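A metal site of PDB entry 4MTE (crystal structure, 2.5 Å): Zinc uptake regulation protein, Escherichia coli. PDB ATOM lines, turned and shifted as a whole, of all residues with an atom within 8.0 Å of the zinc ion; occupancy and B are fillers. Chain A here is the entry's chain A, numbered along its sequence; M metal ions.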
ATOM      1  N   GLY A  74     -29.188 -30.128 -19.968  1.00  0.00           N
ATOM      2  CA  GLY A  74     -28.856 -29.137 -18.960  1.00  0.00           C
ATOM      3  C   GLY A  74     -29.474 -27.772 -19.172  1.00  0.00           C
ATOM      4  O   GLY A  74     -28.868 -26.760 -18.850  1.00  0.00           O
ATOM      5  N   PHE A  75     -30.695 -27.747 -19.701  1.00  0.00           N
ATOM      6  CA  PHE A  75     -31.318 -26.487 -20.124  1.00  0.00           C
ATOM      7  C   PHE A  75     -32.176 -25.822 -19.054  1.00  0.00           C
ATOM      8  O   PHE A  75     -32.228 -24.589 -18.995  1.00  0.00           O
ATOM      9  CB  PHE A  75     -32.166 -26.714 -21.383  1.00  0.00           C
ATOM     10  CG  PHE A  75     -31.362 -27.182 -22.561  1.00  0.00           C
ATOM     11  CD1 PHE A  75     -30.164 -26.578 -22.875  1.00  0.00           C
ATOM     12  CD2 PHE A  75     -31.803 -28.235 -23.343  1.00  0.00           C
ATOM     13  CE1 PHE A  75     -29.421 -27.005 -23.953  1.00  0.00           C
ATOM     14  CE2 PHE A  75     -31.057 -28.670 -24.425  1.00  0.00           C
ATOM     15  CZ  PHE A  75     -29.863 -28.049 -24.731  1.00  0.00           C
ATOM     16  N   VAL A  76     -32.835 -26.615 -18.215  1.00  0.00           N
ATOM     17  CA  VAL A  76     -33.684 -26.065 -17.160  1.00  0.00           C
ATOM     18  C   VAL A  76     -33.422 -26.740 -15.824  1.00  0.00           C
ATOM     19  O   VAL A  76     -32.942 -27.873 -15.761  1.00  0.00           O
ATOM     20  CB  VAL A  76     -35.185 -26.174 -17.507  1.00  0.00           C
ATOM     21  CG1 VAL A  76     -35.449 -25.656 -18.914  1.00  0.00           C
ATOM     22  CG2 VAL A  76     -35.700 -27.603 -17.356  1.00  0.00           C
ATOM     23  N   HIS A  77     -33.722 -26.011 -14.760  1.00  0.00           N
ATOM     24  CA  HIS A  77     -33.692 -26.541 -13.405  1.00  0.00           C
ATOM     25  C   HIS A  77     -35.090 -26.446 -12.825  1.00  0.00           C
ATOM     26  O   HIS A  77     -35.839 -25.501 -13.112  1.00  0.00           O
ATOM     27  CB  HIS A  77     -32.754 -25.732 -12.529  1.00  0.00           C
ATOM     28  CG  HIS A  77     -31.331 -25.760 -12.977  1.00  0.00           C
ATOM     29  ND1 HIS A  77     -30.595 -26.916 -13.060  1.00  0.00           N
ATOM     30  CD2 HIS A  77     -30.507 -24.758 -13.372  1.00  0.00           C
ATOM     31  CE1 HIS A  77     -29.380 -26.638 -13.486  1.00  0.00           C
ATOM     32  NE2 HIS A  77     -29.297 -25.335 -13.684  1.00  0.00           N
ATOM     33  N   VAL A  86     -37.100 -23.152 -14.221  1.00  0.00           N
ATOM     34  CA  VAL A  86     -36.392 -22.006 -14.782  1.00  0.00           C
ATOM     35  C   VAL A  86     -35.240 -22.444 -15.677  1.00  0.00           C
ATOM     36  O   VAL A  86     -34.732 -23.561 -15.539  1.00  0.00           O
ATOM     37  CB  VAL A  86     -35.874 -21.084 -13.642  1.00  0.00           C
ATOM     38  CG1 VAL A  86     -34.872 -21.828 -12.760  1.00  0.00           C
ATOM     39  CG2 VAL A  86     -35.286 -19.783 -14.205  1.00  0.00           C
ATOM     40  N   LEU A  87     -34.836 -21.578 -16.593  1.00  0.00           N
ATOM     41  CA  LEU A  87     -33.667 -21.826 -17.431  1.00  0.00           C
ATOM     42  C   LEU A  87     -32.383 -21.785 -16.630  1.00  0.00           C
ATOM     43  O   LEU A  87     -32.255 -21.022 -15.660  1.00  0.00           O
ATOM     44  CB  LEU A  87     -33.561 -20.775 -18.539  1.00  0.00           C
ATOM     45  CG  LEU A  87     -34.450 -20.874 -19.779  1.00  0.00           C
ATOM     46  CD1 LEU A  87     -33.831 -20.040 -20.889  1.00  0.00           C
ATOM     47  CD2 LEU A  87     -34.660 -22.299 -20.239  1.00  0.00           C
ATOM     48  N   CYS A  88     -31.414 -22.601 -17.045  1.00  0.00           N
ATOM     49  CA  CYS A  88     -30.060 -22.515 -16.523  1.00  0.00           C
ATOM     50  C   CYS A  88     -29.334 -21.380 -17.246  1.00  0.00           C
ATOM     51  O   CYS A  88     -29.569 -21.150 -18.435  1.00  0.00           O
ATOM     52  CB  CYS A  88     -29.333 -23.840 -16.754  1.00  0.00           C
ATOM     53  SG  CYS A  88     -27.622 -23.836 -16.186  1.00  0.00           S
ATOM     54  N   HIS A  89     -28.451 -20.680 -16.543  1.00  0.00           N
ATOM     55  CA  HIS A  89     -27.757 -19.521 -17.115  1.00  0.00           C
ATOM     56  C   HIS A  89     -26.592 -19.942 -18.015  1.00  0.00           C
ATOM     57  O   HIS A  89     -26.054 -19.127 -18.764  1.00  0.00           O
ATOM     58  CB  HIS A  89     -27.270 -18.587 -16.012  1.00  0.00           C
ATOM     59  CG  HIS A  89     -26.212 -19.178 -15.142  1.00  0.00           C
ATOM     60  ND1 HIS A  89     -26.441 -20.278 -14.345  1.00  0.00           N
ATOM     61  CD2 HIS A  89     -24.922 -18.810 -14.917  1.00  0.00           C
ATOM     62  CE1 HIS A  89     -25.334 -20.578 -13.689  1.00  0.00           C
ATOM     63  NE2 HIS A  89     -24.400 -19.700 -14.012  1.00  0.00           N
ATOM     64  N   LEU A  90     -26.188 -21.208 -17.918  1.00  0.00           N
ATOM     65  CA  LEU A  90     -25.119 -21.753 -18.766  1.00  0.00           C
ATOM     66  C   LEU A  90     -25.442 -23.202 -19.157  1.00  0.00           C
ATOM     67  O   LEU A  90     -25.597 -24.059 -18.292  1.00  0.00           O
ATOM     68  CB  LEU A  90     -23.774 -21.675 -18.042  1.00  0.00           C
ATOM     69  CG  LEU A  90     -22.562 -22.142 -18.848  1.00  0.00           C
ATOM     70  CD1 LEU A  90     -22.357 -21.276 -20.092  1.00  0.00           C
ATOM     71  CD2 LEU A  90     -21.317 -22.134 -17.973  1.00  0.00           C
ATOM     72  N   PHE A  91     -25.510 -23.459 -20.456  1.00  0.00           N
ATOM     73  CA  PHE A  91     -26.110 -24.696 -20.968  1.00  0.00           C
ATOM     74  C   PHE A  91     -25.199 -25.922 -21.015  1.00  0.00           C
ATOM     75  O   PHE A  91     -25.487 -26.934 -20.380  1.00  0.00           O
ATOM     76  CB  PHE A  91     -26.702 -24.434 -22.363  1.00  0.00           C
ATOM     77  CG  PHE A  91     -28.041 -23.755 -22.350  1.00  0.00           C
ATOM     78  CD1 PHE A  91     -28.536 -23.164 -21.198  1.00  0.00           C
ATOM     79  CD2 PHE A  91     -28.820 -23.704 -23.501  1.00  0.00           C
ATOM     80  CE1 PHE A  91     -29.771 -22.548 -21.196  1.00  0.00           C
ATOM     81  CE2 PHE A  91     -30.051 -23.081 -23.487  1.00  0.00           C
ATOM     82  CZ  PHE A  91     -30.528 -22.507 -22.340  1.00  0.00           C
ATOM     83  N   GLN A  93     -22.768 -27.367 -19.842  1.00  0.00           N
ATOM     84  CA  GLN A  93     -22.054 -28.006 -18.739  1.00  0.00           C
ATOM     85  C   GLN A  93     -22.844 -29.192 -18.177  1.00  0.00           C
ATOM     86  O   GLN A  93     -24.069 -29.234 -18.303  1.00  0.00           O
ATOM     87  CB  GLN A  93     -21.741 -26.993 -17.644  1.00  0.00           C
ATOM     88  CG  GLN A  93     -22.959 -26.405 -16.953  1.00  0.00           C
ATOM     89  CD  GLN A  93     -22.584 -25.318 -15.964  1.00  0.00           C
ATOM     90  OE1 GLN A  93     -21.439 -24.900 -15.884  1.00  0.00           O
ATOM     91  NE2 GLN A  93     -23.571 -24.854 -15.193  1.00  0.00           N
ATOM     92  N   PRO A  94     -22.137 -30.169 -17.577  1.00  0.00           N
ATOM     93  CA  PRO A  94     -22.781 -31.386 -17.075  1.00  0.00           C
ATOM     94  C   PRO A  94     -23.499 -31.181 -15.730  1.00  0.00           C
ATOM     95  O   PRO A  94     -23.647 -30.045 -15.294  1.00  0.00           O
ATOM     96  CB  PRO A  94     -21.608 -32.352 -16.911  1.00  0.00           C
ATOM     97  CG  PRO A  94     -20.466 -31.467 -16.582  1.00  0.00           C
ATOM     98  CD  PRO A  94     -20.674 -30.198 -17.361  1.00  0.00           C
ATOM     99  N   THR A  95     -23.927 -32.271 -15.113  1.00  0.00           N
ATOM    100  CA  THR A  95     -24.673 -32.222 -13.857  1.00  0.00           C
ATOM    101  C   THR A  95     -23.922 -31.410 -12.805  1.00  0.00           C
ATOM    102  O   THR A  95     -22.888 -31.841 -12.288  1.00  0.00           O
ATOM    103  CB  THR A  95     -24.920 -33.639 -13.300  1.00  0.00           C
ATOM    104  OG1 THR A  95     -23.672 -34.311 -13.106  1.00  0.00           O
ATOM    105  CG2 THR A  95     -25.785 -34.440 -14.258  1.00  0.00           C
ATOM    106  N   HIS A  96     -24.448 -30.235 -12.503  1.00  0.00           N
ATOM    107  CA  HIS A  96     -23.791 -29.289 -11.611  1.00  0.00           C
ATOM    108  C   HIS A  96     -24.706 -28.875 -10.465  1.00  0.00           C
ATOM    109  O   HIS A  96     -25.917 -28.708 -10.645  1.00  0.00           O
ATOM    110  CB  HIS A  96     -23.343 -28.054 -12.384  1.00  0.00           C
ATOM    111  CG  HIS A  96     -24.464 -27.321 -13.056  1.00  0.00           C
ATOM    112  ND1 HIS A  96     -25.112 -27.810 -14.172  1.00  0.00           N
ATOM    113  CD2 HIS A  96     -25.059 -26.139 -12.775  1.00  0.00           C
ATOM    114  CE1 HIS A  96     -26.048 -26.964 -14.549  1.00  0.00           C
ATOM    115  NE2 HIS A  96     -26.036 -25.939 -13.710  1.00  0.00           N
ATOM    116  N   THR A  97     -24.103 -28.704  -9.291  1.00  0.00           N
ATOM    117  CA  THR A  97     -24.798 -28.117  -8.150  1.00  0.00           C
ATOM    118  C   THR A  97     -24.680 -26.605  -8.248  1.00  0.00           C
ATOM    119  O   THR A  97     -23.574 -26.073  -8.379  1.00  0.00           O
ATOM    120  CB  THR A  97     -24.177 -28.591  -6.818  1.00  0.00           C
ATOM    121  OG1 THR A  97     -24.490 -29.983  -6.607  1.00  0.00           O
ATOM    122  CG2 THR A  97     -24.705 -27.774  -5.636  1.00  0.00           C
ATOM    123  N   SER A  98     -25.816 -25.923  -8.199  1.00  0.00           N
ATOM    124  CA  SER A  98     -25.837 -24.467  -8.216  1.00  0.00           C
ATOM    125  C   SER A  98     -26.793 -23.945  -7.150  1.00  0.00           C
ATOM    126  O   SER A  98     -27.788 -24.585  -6.812  1.00  0.00           O
ATOM    127  CB  SER A  98     -26.262 -23.945  -9.587  1.00  0.00           C
ATOM    128  OG  SER A  98     -25.173 -23.950 -10.497  1.00  0.00           O
ATOM    129  N   ALA A  99     -26.467 -22.769  -6.608  1.00  0.00           N
ATOM    130  CA  ALA A  99     -27.283 -22.127  -5.591  1.00  0.00           C
ATOM    131  C   ALA A  99     -28.296 -21.202  -6.265  1.00  0.00           C
ATOM    132  O   ALA A  99     -27.921 -20.389  -7.107  1.00  0.00           O
ATOM    133  CB  ALA A  99     -26.408 -21.362  -4.625  1.00  0.00           C
ATOM    134  N   MET A 100     -29.563 -21.334  -5.884  1.00  0.00           N
ATOM    135  CA  MET A 100     -30.647 -20.576  -6.499  1.00  0.00           C
ATOM    136  C   MET A 100     -31.123 -19.449  -5.593  1.00  0.00           C
ATOM    137  O   MET A 100     -31.594 -19.712  -4.481  1.00  0.00           O
ATOM    138  CB  MET A 100     -31.819 -21.508  -6.791  1.00  0.00           C
ATOM    139  CG  MET A 100     -31.544 -22.516  -7.894  1.00  0.00           C
ATOM    140  SD  MET A 100     -31.485 -21.747  -9.524  1.00  0.00           S
ATOM    141  CE  MET A 100     -31.166 -23.161 -10.561  1.00  0.00           C
ATOM    142  N   GLU A 111     -28.751 -17.808 -10.543  1.00  0.00           N
ATOM    143  CA  GLU A 111     -28.041 -19.059 -10.318  1.00  0.00           C
ATOM    144  C   GLU A 111     -26.547 -18.796 -10.182  1.00  0.00           C
ATOM    145  O   GLU A 111     -25.912 -18.324 -11.113  1.00  0.00           O
ATOM    146  CB  GLU A 111     -28.303 -20.014 -11.489  1.00  0.00           C
ATOM    147  CG  GLU A 111     -27.730 -21.405 -11.288  1.00  0.00           C
ATOM    148  CD  GLU A 111     -27.880 -22.299 -12.517  1.00  0.00           C
ATOM    149  OE1 GLU A 111     -27.245 -23.367 -12.545  1.00  0.00           O
ATOM    150  OE2 GLU A 111     -28.633 -21.934 -13.437  1.00  0.00           O
ATOM    151  N   GLU A 112     -26.004 -19.103  -8.999  1.00  0.00           N
ATOM    152  CA  GLU A 112     -24.578 -18.903  -8.736  1.00  0.00           C
ATOM    153  C   GLU A 112     -23.922 -20.190  -8.242  1.00  0.00           C
ATOM    154  O   GLU A 112     -24.594 -21.155  -7.905  1.00  0.00           O
ATOM    155  CB  GLU A 112     -24.374 -17.796  -7.697  1.00  0.00           C
ATOM    156  CG  GLU A 112     -24.911 -16.443  -8.134  1.00  0.00           C
ATOM    157  CD  GLU A 112     -23.873 -15.346  -8.040  1.00  0.00           C
ATOM    158  OE1 GLU A 112     -23.166 -15.263  -7.014  1.00  0.00           O
ATOM    159  OE2 GLU A 112     -23.747 -14.559  -9.007  1.00  0.00           O
HETATM  160 ZN    ZN M   1     -27.510 -24.562 -14.115  1.00  0.00          ZN
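The backbone carbonyl oxygen (O) of Val 86 lies within hydrogen-bond range of the backbone NH (N) of His 77 (2.8 Å).
The side-chain amide nitrogen (NE2) of Gln 93 lies close to a ring nitrogen (ND1) of His 96, at 3.5 Å.
The side-chain sulfur (SG) of Cys 88 sits close to the backbone carbonyl oxygen (O) of Leu 90.
N of Cys 88 is in hydrogen-bond range of O of Phe 75 (2.9 Å).
OE2 of Glu 111 is in hydrogen-bond range of ND1 of His 89 (2.9 Å).
A ring nitrogen (ND1) of His 96 lies within hydrogen-bond range of the backbone carbonyl oxygen (O) of Pro 94 (2.9 Å).
The side-chain carboxylate (OE1) of Glu 111 sits close to the side-chain hydroxyl (OG) of Ser 98.
Within 4 Å of the zinc ion: His 77, Cys 88, His 96 and Glu 111.
The zinc ion is bound by OE1 of Glu 111 (2.0 Å), NE2 of His 77 (2.0 Å), NE2 of His 96 (2.1 Å) and SG of Cys 88 (2.2 Å).
The zinc ion has four donor atoms within binding distance.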
